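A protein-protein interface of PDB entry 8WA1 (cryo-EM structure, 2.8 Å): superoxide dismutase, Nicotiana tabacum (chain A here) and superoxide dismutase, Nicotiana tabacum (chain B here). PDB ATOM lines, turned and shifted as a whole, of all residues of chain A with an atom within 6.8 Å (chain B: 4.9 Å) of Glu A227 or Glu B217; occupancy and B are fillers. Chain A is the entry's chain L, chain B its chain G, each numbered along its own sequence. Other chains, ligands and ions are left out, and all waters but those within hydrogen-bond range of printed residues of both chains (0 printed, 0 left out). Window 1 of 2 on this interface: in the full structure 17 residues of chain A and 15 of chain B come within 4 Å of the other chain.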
ATOM      1  N   HIS A  77     -36.941  19.430   6.442  1.00  0.00           N
ATOM      2  CA  HIS A  77     -36.968  20.593   5.599  1.00  0.00           C
ATOM      3  C   HIS A  77     -38.216  21.397   5.755  1.00  0.00           C
ATOM      4  O   HIS A  77     -38.162  22.604   5.980  1.00  0.00           O
ATOM      5  CB  HIS A  77     -36.622  20.217   4.165  1.00  0.00           C
ATOM      6  CG  HIS A  77     -35.195  19.792   4.017  1.00  0.00           C
ATOM      7  ND1 HIS A  77     -34.170  20.694   3.829  1.00  0.00           N
ATOM      8  CD2 HIS A  77     -34.610  18.573   4.104  1.00  0.00           C
ATOM      9  CE1 HIS A  77     -33.021  20.046   3.774  1.00  0.00           C
ATOM     10  NE2 HIS A  77     -33.260  18.757   3.934  1.00  0.00           N
ATOM     11  N   GLY A 171     -25.085  21.472  -8.588  1.00  0.00           N
ATOM     12  CA  GLY A 171     -25.238  22.007  -7.252  1.00  0.00           C
ATOM     13  C   GLY A 171     -26.638  21.884  -6.695  1.00  0.00           C
ATOM     14  O   GLY A 171     -27.304  20.860  -6.878  1.00  0.00           O
ATOM     15  N   SER A 172     -27.114  22.931  -6.044  1.00  0.00           N
ATOM     16  CA  SER A 172     -28.436  22.895  -5.449  1.00  0.00           C
ATOM     17  C   SER A 172     -29.472  23.497  -6.387  1.00  0.00           C
ATOM     18  O   SER A 172     -29.414  24.681  -6.705  1.00  0.00           O
ATOM     19  CB  SER A 172     -28.408  23.665  -4.139  1.00  0.00           C
ATOM     20  OG  SER A 172     -27.422  23.145  -3.269  1.00  0.00           O
ATOM     21  N   GLY A 173     -30.413  22.684  -6.847  1.00  0.00           N
ATOM     22  CA  GLY A 173     -31.417  23.177  -7.770  1.00  0.00           C
ATOM     23  C   GLY A 173     -32.695  22.382  -7.889  1.00  0.00           C
ATOM     24  O   GLY A 173     -32.791  21.280  -7.374  1.00  0.00           O
ATOM     25  N   ASP A 224     -36.661  17.482  -7.345  1.00  0.00           N
ATOM     26  CA  ASP A 224     -35.818  18.176  -6.397  1.00  0.00           C
ATOM     27  C   ASP A 224     -34.431  17.632  -6.568  1.00  0.00           C
ATOM     28  O   ASP A 224     -34.099  16.589  -6.009  1.00  0.00           O
ATOM     29  CB  ASP A 224     -36.281  17.897  -4.974  1.00  0.00           C
ATOM     30  CG  ASP A 224     -35.522  18.695  -3.946  1.00  0.00           C
ATOM     31  OD1 ASP A 224     -34.957  19.740  -4.308  1.00  0.00           O
ATOM     32  OD2 ASP A 224     -35.504  18.285  -2.773  1.00  0.00           O
ATOM     33  N   VAL A 225     -33.610  18.327  -7.344  1.00  0.00           N
ATOM     34  CA  VAL A 225     -32.232  17.906  -7.496  1.00  0.00           C
ATOM     35  C   VAL A 225     -31.377  18.541  -6.430  1.00  0.00           C
ATOM     36  O   VAL A 225     -30.593  19.435  -6.708  1.00  0.00           O
ATOM     37  CB  VAL A 225     -31.693  18.178  -8.903  1.00  0.00           C
ATOM     38  CG1 VAL A 225     -31.577  16.868  -9.659  1.00  0.00           C
ATOM     39  CG2 VAL A 225     -32.617  19.113  -9.661  1.00  0.00           C
ATOM     40  N   TRP A 226     -31.534  18.084  -5.203  1.00  0.00           N
ATOM     41  CA  TRP A 226     -30.735  18.586  -4.114  1.00  0.00           C
ATOM     42  C   TRP A 226     -30.236  17.308  -3.535  1.00  0.00           C
ATOM     43  O   TRP A 226     -30.853  16.264  -3.703  1.00  0.00           O
ATOM     44  CB  TRP A 226     -31.578  19.303  -3.076  1.00  0.00           C
ATOM     45  CG  TRP A 226     -31.790  20.764  -3.310  1.00  0.00           C
ATOM     46  CD1 TRP A 226     -32.369  21.343  -4.392  1.00  0.00           C
ATOM     47  CD2 TRP A 226     -31.456  21.830  -2.417  1.00  0.00           C
ATOM     48  NE1 TRP A 226     -32.403  22.705  -4.243  1.00  0.00           N
ATOM     49  CE2 TRP A 226     -31.849  23.030  -3.035  1.00  0.00           C
ATOM     50  CE3 TRP A 226     -30.854  21.887  -1.160  1.00  0.00           C
ATOM     51  CZ2 TRP A 226     -31.661  24.271  -2.441  1.00  0.00           C
ATOM     52  CZ3 TRP A 226     -30.670  23.121  -0.569  1.00  0.00           C
ATOM     53  CH2 TRP A 226     -31.071  24.297  -1.210  1.00  0.00           C
ATOM     54  N   GLU A 227     -29.120  17.368  -2.846  1.00  0.00           N
ATOM     55  CA  GLU A 227     -28.522  16.155  -2.327  1.00  0.00           C
ATOM     56  C   GLU A 227     -29.403  15.436  -1.338  1.00  0.00           C
ATOM     57  O   GLU A 227     -29.464  14.217  -1.345  1.00  0.00           O
ATOM     58  CB  GLU A 227     -27.147  16.444  -1.726  1.00  0.00           C
ATOM     59  CG  GLU A 227     -26.000  16.272  -2.707  1.00  0.00           C
ATOM     60  CD  GLU A 227     -25.015  17.420  -2.656  1.00  0.00           C
ATOM     61  OE1 GLU A 227     -25.381  18.494  -2.136  1.00  0.00           O
ATOM     62  OE2 GLU A 227     -23.878  17.253  -3.146  1.00  0.00           O
ATOM     63  N   HIS A 228     -30.143  16.169  -0.524  1.00  0.00           N
ATOM     64  CA  HIS A 228     -30.892  15.501   0.519  1.00  0.00           C
ATOM     65  C   HIS A 228     -31.825  14.465  -0.048  1.00  0.00           C
ATOM     66  O   HIS A 228     -32.027  13.420   0.560  1.00  0.00           O
ATOM     67  CB  HIS A 228     -31.638  16.487   1.422  1.00  0.00           C
ATOM     68  CG  HIS A 228     -32.408  17.551   0.703  1.00  0.00           C
ATOM     69  ND1 HIS A 228     -32.277  18.887   1.005  1.00  0.00           N
ATOM     70  CD2 HIS A 228     -33.349  17.478  -0.266  1.00  0.00           C
ATOM     71  CE1 HIS A 228     -33.092  19.594   0.244  1.00  0.00           C
ATOM     72  NE2 HIS A 228     -33.752  18.762  -0.540  1.00  0.00           N
ATOM     73  N   ALA A 229     -32.386  14.729  -1.213  1.00  0.00           N
ATOM     74  CA  ALA A 229     -33.358  13.815  -1.773  1.00  0.00           C
ATOM     75  C   ALA A 229     -32.807  12.427  -2.035  1.00  0.00           C
ATOM     76  O   ALA A 229     -33.473  11.441  -1.747  1.00  0.00           O
ATOM     77  CB  ALA A 229     -33.922  14.393  -3.057  1.00  0.00           C
ATOM     78  N   TYR A 230     -31.589  12.322  -2.547  1.00  0.00           N
ATOM     79  CA  TYR A 230     -31.081  11.003  -2.930  1.00  0.00           C
ATOM     80  C   TYR A 230     -29.791  10.577  -2.264  1.00  0.00           C
ATOM     81  O   TYR A 230     -29.473   9.392  -2.235  1.00  0.00           O
ATOM     82  CB  TYR A 230     -30.882  10.961  -4.443  1.00  0.00           C
ATOM     83  CG  TYR A 230     -29.745  11.843  -4.914  1.00  0.00           C
ATOM     84  CD1 TYR A 230     -29.907  13.217  -5.019  1.00  0.00           C
ATOM     85  CD2 TYR A 230     -28.509  11.302  -5.241  1.00  0.00           C
ATOM     86  CE1 TYR A 230     -28.873  14.026  -5.432  1.00  0.00           C
ATOM     87  CE2 TYR A 230     -27.470  12.105  -5.656  1.00  0.00           C
ATOM     88  CZ  TYR A 230     -27.660  13.465  -5.750  1.00  0.00           C
ATOM     89  OH  TYR A 230     -26.632  14.273  -6.170  1.00  0.00           O
ATOM     90  N   TYR A 231     -29.031  11.533  -1.752  1.00  0.00           N
ATOM     91  CA  TYR A 231     -27.737  11.206  -1.168  1.00  0.00           C
ATOM     92  C   TYR A 231     -27.935  10.293   0.017  1.00  0.00           C
ATOM     93  O   TYR A 231     -27.174   9.351   0.221  1.00  0.00           O
ATOM     94  CB  TYR A 231     -27.017  12.479  -0.720  1.00  0.00           C
ATOM     95  CG  TYR A 231     -25.642  12.263  -0.141  1.00  0.00           C
ATOM     96  CD1 TYR A 231     -24.531  12.214  -0.961  1.00  0.00           C
ATOM     97  CD2 TYR A 231     -25.454  12.124   1.224  1.00  0.00           C
ATOM     98  CE1 TYR A 231     -23.268  12.016  -0.443  1.00  0.00           C
ATOM     99  CE2 TYR A 231     -24.195  11.930   1.750  1.00  0.00           C
ATOM    100  CZ  TYR A 231     -23.106  11.873   0.914  1.00  0.00           C
ATOM    101  OH  TYR A 231     -21.847  11.678   1.429  1.00  0.00           O
ATOM    102  N   LEU A 232     -28.949  10.580   0.814  1.00  0.00           N
ATOM    103  CA  LEU A 232     -29.180   9.781   1.994  1.00  0.00           C
ATOM    104  C   LEU A 232     -29.753   8.470   1.544  1.00  0.00           C
ATOM    105  O   LEU A 232     -29.245   7.411   1.903  1.00  0.00           O
ATOM    106  CB  LEU A 232     -30.159  10.488   2.922  1.00  0.00           C
ATOM    107  CG  LEU A 232     -30.048  10.153   4.410  1.00  0.00           C
ATOM    108  CD1 LEU A 232     -30.868   8.933   4.799  1.00  0.00           C
ATOM    109  CD2 LEU A 232     -28.591   9.998   4.819  1.00  0.00           C
ATOM    110  N   ASP A 233     -30.806   8.538   0.747  1.00  0.00           N
ATOM    111  CA  ASP A 233     -31.473   7.333   0.301  1.00  0.00           C
ATOM    112  C   ASP A 233     -30.526   6.306  -0.244  1.00  0.00           C
ATOM    113  O   ASP A 233     -30.461   5.185   0.250  1.00  0.00           O
ATOM    114  CB  ASP A 233     -32.448   7.715  -0.812  1.00  0.00           C
ATOM    115  CG  ASP A 233     -33.362   6.578  -1.212  1.00  0.00           C
ATOM    116  OD1 ASP A 233     -33.672   5.721  -0.358  1.00  0.00           O
ATOM    117  OD2 ASP A 233     -33.786   6.554  -2.385  1.00  0.00           O
ATOM    118  N   ASN A 236     -24.697   8.082  -3.819  1.00  0.00           N
ATOM    119  CA  ASN A 236     -24.997   9.301  -4.558  1.00  0.00           C
ATOM    120  C   ASN A 236     -24.683   9.319  -6.031  1.00  0.00           C
ATOM    121  O   ASN A 236     -23.764  10.010  -6.472  1.00  0.00           O
ATOM    122  CB  ASN A 236     -24.321  10.492  -3.883  1.00  0.00           C
ATOM    123  CG  ASN A 236     -22.938  10.159  -3.360  1.00  0.00           C
ATOM    124  OD1 ASN A 236     -22.787   9.412  -2.394  1.00  0.00           O
ATOM    125  ND2 ASN A 236     -21.921  10.729  -3.987  1.00  0.00           N
ATOM    126  N   ARG A 238     -26.589  10.511  -9.077  1.00  0.00           N
ATOM    127  CA  ARG A 238     -27.836  11.219  -9.335  1.00  0.00           C
ATOM    128  C   ARG A 238     -28.613  10.649 -10.536  1.00  0.00           C
ATOM    129  O   ARG A 238     -29.840  10.605 -10.481  1.00  0.00           O
ATOM    130  CB  ARG A 238     -27.602  12.731  -9.482  1.00  0.00           C
ATOM    131  CG  ARG A 238     -28.873  13.561  -9.371  1.00  0.00           C
ATOM    132  CD  ARG A 238     -28.600  14.987  -8.916  1.00  0.00           C
ATOM    133  NE  ARG A 238     -27.997  15.822  -9.950  1.00  0.00           N
ATOM    134  CZ  ARG A 238     -27.710  17.109  -9.787  1.00  0.00           C
ATOM    135  NH1 ARG A 238     -27.163  17.803 -10.774  1.00  0.00           N
ATOM    136  NH2 ARG A 238     -27.974  17.708  -8.633  1.00  0.00           N
ATOM    137  N   SER B 177     -25.186  25.254  -1.397  1.00  0.00           N
ATOM    138  CA  SER B 177     -23.884  24.600  -1.492  1.00  0.00           C
ATOM    139  C   SER B 177     -22.822  25.632  -1.798  1.00  0.00           C
ATOM    140  O   SER B 177     -23.069  26.570  -2.547  1.00  0.00           O
ATOM    141  CB  SER B 177     -23.912  23.552  -2.593  1.00  0.00           C
ATOM    142  OG  SER B 177     -24.753  22.472  -2.240  1.00  0.00           O
ATOM    143  N   LEU B 215     -19.182  23.242   2.110  1.00  0.00           N
ATOM    144  CA  LEU B 215     -20.549  23.376   2.573  1.00  0.00           C
ATOM    145  C   LEU B 215     -21.467  22.653   1.629  1.00  0.00           C
ATOM    146  O   LEU B 215     -22.680  22.728   1.765  1.00  0.00           O
ATOM    147  CB  LEU B 215     -20.958  24.833   2.711  1.00  0.00           C
ATOM    148  CG  LEU B 215     -20.224  25.588   3.814  1.00  0.00           C
ATOM    149  CD1 LEU B 215     -20.774  26.998   3.928  1.00  0.00           C
ATOM    150  CD2 LEU B 215     -20.372  24.852   5.135  1.00  0.00           C
ATOM    151  N   TRP B 216     -20.908  21.973   0.643  1.00  0.00           N
ATOM    152  CA  TRP B 216     -21.756  21.169  -0.207  1.00  0.00           C
ATOM    153  C   TRP B 216     -22.264  20.052   0.684  1.00  0.00           C
ATOM    154  O   TRP B 216     -21.524  19.535   1.514  1.00  0.00           O
ATOM    155  CB  TRP B 216     -21.001  20.627  -1.412  1.00  0.00           C
ATOM    156  CG  TRP B 216     -20.760  21.627  -2.490  1.00  0.00           C
ATOM    157  CD1 TRP B 216     -20.155  22.838  -2.362  1.00  0.00           C
ATOM    158  CD2 TRP B 216     -21.101  21.494  -3.873  1.00  0.00           C
ATOM    159  NE1 TRP B 216     -20.108  23.475  -3.574  1.00  0.00           N
ATOM    160  CE2 TRP B 216     -20.681  22.670  -4.521  1.00  0.00           C
ATOM    161  CE3 TRP B 216     -21.728  20.498  -4.625  1.00  0.00           C
ATOM    162  CZ2 TRP B 216     -20.865  22.876  -5.885  1.00  0.00           C
ATOM    163  CZ3 TRP B 216     -21.906  20.704  -5.979  1.00  0.00           C
ATOM    164  CH2 TRP B 216     -21.477  21.883  -6.595  1.00  0.00           C
ATOM    165  N   GLU B 217     -23.511  19.651   0.506  1.00  0.00           N
ATOM    166  CA  GLU B 217     -24.111  18.650   1.382  1.00  0.00           C
ATOM    167  C   GLU B 217     -23.452  17.304   1.330  1.00  0.00           C
ATOM    168  O   GLU B 217     -23.458  16.582   2.318  1.00  0.00           O
ATOM    169  CB  GLU B 217     -25.603  18.512   1.107  1.00  0.00           C
ATOM    170  CG  GLU B 217     -26.356  19.830   1.149  1.00  0.00           C
ATOM    171  CD  GLU B 217     -27.840  19.663   0.915  1.00  0.00           C
ATOM    172  OE1 GLU B 217     -28.286  18.521   0.687  1.00  0.00           O
ATOM    173  OE2 GLU B 217     -28.565  20.678   0.960  1.00  0.00           O
ATOM    174  N   HIS B 218     -22.863  16.957   0.197  1.00  0.00           N
ATOM    175  CA  HIS B 218     -22.312  15.627   0.071  1.00  0.00           C
ATOM    176  C   HIS B 218     -21.283  15.396   1.145  1.00  0.00           C
ATOM    177  O   HIS B 218     -21.095  14.281   1.602  1.00  0.00           O
ATOM    178  CB  HIS B 218     -21.737  15.347  -1.316  1.00  0.00           C
ATOM    179  CG  HIS B 218     -20.791  16.390  -1.831  1.00  0.00           C
ATOM    180  ND1 HIS B 218     -20.948  16.983  -3.064  1.00  0.00           N
ATOM    181  CD2 HIS B 218     -19.660  16.915  -1.305  1.00  0.00           C
ATOM    182  CE1 HIS B 218     -19.963  17.839  -3.269  1.00  0.00           C
ATOM    183  NE2 HIS B 218     -19.170  17.821  -2.213  1.00  0.00           N
ATOM    184  N   ALA B 219     -20.593  16.445   1.540  1.00  0.00           N
ATOM    185  CA  ALA B 219     -19.626  16.308   2.596  1.00  0.00           C
ATOM    186  C   ALA B 219     -20.214  15.889   3.926  1.00  0.00           C
ATOM    187  O   ALA B 219     -19.654  15.031   4.601  1.00  0.00           O
ATOM    188  CB  ALA B 219     -18.892  17.618   2.770  1.00  0.00           C
ATOM    189  N   TYR B 220     -21.339  16.467   4.324  1.00  0.00           N
ATOM    190  CA  TYR B 220     -21.843  16.168   5.665  1.00  0.00           C
ATOM    191  C   TYR B 220     -23.079  15.306   5.860  1.00  0.00           C
ATOM    192  O   TYR B 220     -23.287  14.811   6.959  1.00  0.00           O
ATOM    193  CB  TYR B 220     -22.037  17.472   6.445  1.00  0.00           C
ATOM    194  CG  TYR B 220     -23.040  18.427   5.845  1.00  0.00           C
ATOM    195  CD1 TYR B 220     -24.393  18.304   6.117  1.00  0.00           C
ATOM    196  CD2 TYR B 220     -22.630  19.465   5.026  1.00  0.00           C
ATOM    197  CE1 TYR B 220     -25.313  19.174   5.574  1.00  0.00           C
ATOM    198  CE2 TYR B 220     -23.543  20.345   4.482  1.00  0.00           C
ATOM    199  CZ  TYR B 220     -24.881  20.192   4.759  1.00  0.00           C
ATOM    200  OH  TYR B 220     -25.796  21.063   4.221  1.00  0.00           O
ATOM    201  N   TYR B 221     -23.863  15.050   4.822  1.00  0.00           N
ATOM    202  CA  TYR B 221     -25.140  14.351   5.033  1.00  0.00           C
ATOM    203  C   TYR B 221     -25.058  12.952   5.624  1.00  0.00           C
ATOM    204  O   TYR B 221     -25.856  12.607   6.490  1.00  0.00           O
ATOM    205  CB  TYR B 221     -25.967  14.326   3.747  1.00  0.00           C
ATOM    206  CG  TYR B 221     -27.411  14.698   3.947  1.00  0.00           C
ATOM    207  CD1 TYR B 221     -28.326  13.774   4.424  1.00  0.00           C
ATOM    208  CD2 TYR B 221     -27.860  15.972   3.654  1.00  0.00           C
ATOM    209  CE1 TYR B 221     -29.650  14.114   4.611  1.00  0.00           C
ATOM    210  CE2 TYR B 221     -29.181  16.321   3.837  1.00  0.00           C
ATOM    211  CZ  TYR B 221     -30.071  15.388   4.319  1.00  0.00           C
ATOM    212  OH  TYR B 221     -31.389  15.733   4.508  1.00  0.00           O
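NE2 of His A77 touches OH of Tyr B221 (3.6 Å).
Gly A171 touches Trp B216.
Trp A226 touches Glu B217 (CE3 to OE2, 3.3 Å).
CB of His A228 touches OH of Tyr B221, 3.2 Å away.
Tyr B221 touches Tyr A231 (CB to CD2, 3.4 Å).
Tyr B221 touches Leu A232.
OG of Ser B177 sits at hydrogen-bond distance from OG of Ser A172 (2.9 Å).
The side-chain carboxylate (OE1) of Glu A227 sits close to the backbone NH (N) of Glu B217 (3.4 Å).
N of His A228 lies within hydrogen-bond range of OE1 of Glu B217 (3.2 Å).
A ring nitrogen (ND1) of His B218 sits at hydrogen-bond distance from the side-chain carboxylate (OE2) of Glu A227 (2.9 Å).
The side-chain hydroxyl of Tyr A231 sits at hydrogen-bond distance from the backbone carbonyl oxygen of His B218 (2.7 Å).
Printed residues of chain B within 4 Å of His A228: Glu B217 (3.2 Å) and Tyr B221 (3.2 Å).
Of the printed residues of chain B, Leu A232 touches Tyr B221.
Of the printed residues of chain A, Trp B216 touches Gly A171.
The nearest residue of chain A that does not touch Glu B217 is Tyr A231 (4.7 Å).
ND1 of His A228 lies close to NE2 of His A77 (3.1 Å).
O of Gly A173 sits close to NE1 of Trp A226, at 3.5 Å.
Of the 8 printed residues of chain B, 5 touch a printed residue of chain A.
Printed residues of chain A that touch a printed residue of chain B: His A77, Gly A171, Ser A172, Trp A226, Glu A227, His A228, Tyr A231 and Leu A232.
Hydrophobic or aromatic side chains of chain A within 4 Å of the printed part of chain B: His A77, Trp A226, His A228, Tyr A231 and Leu A232.
Among the printed residues, no Asp or Glu carboxylate lies within 4 Å of a Lys or Arg side-chain nitrogen of the other chain.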
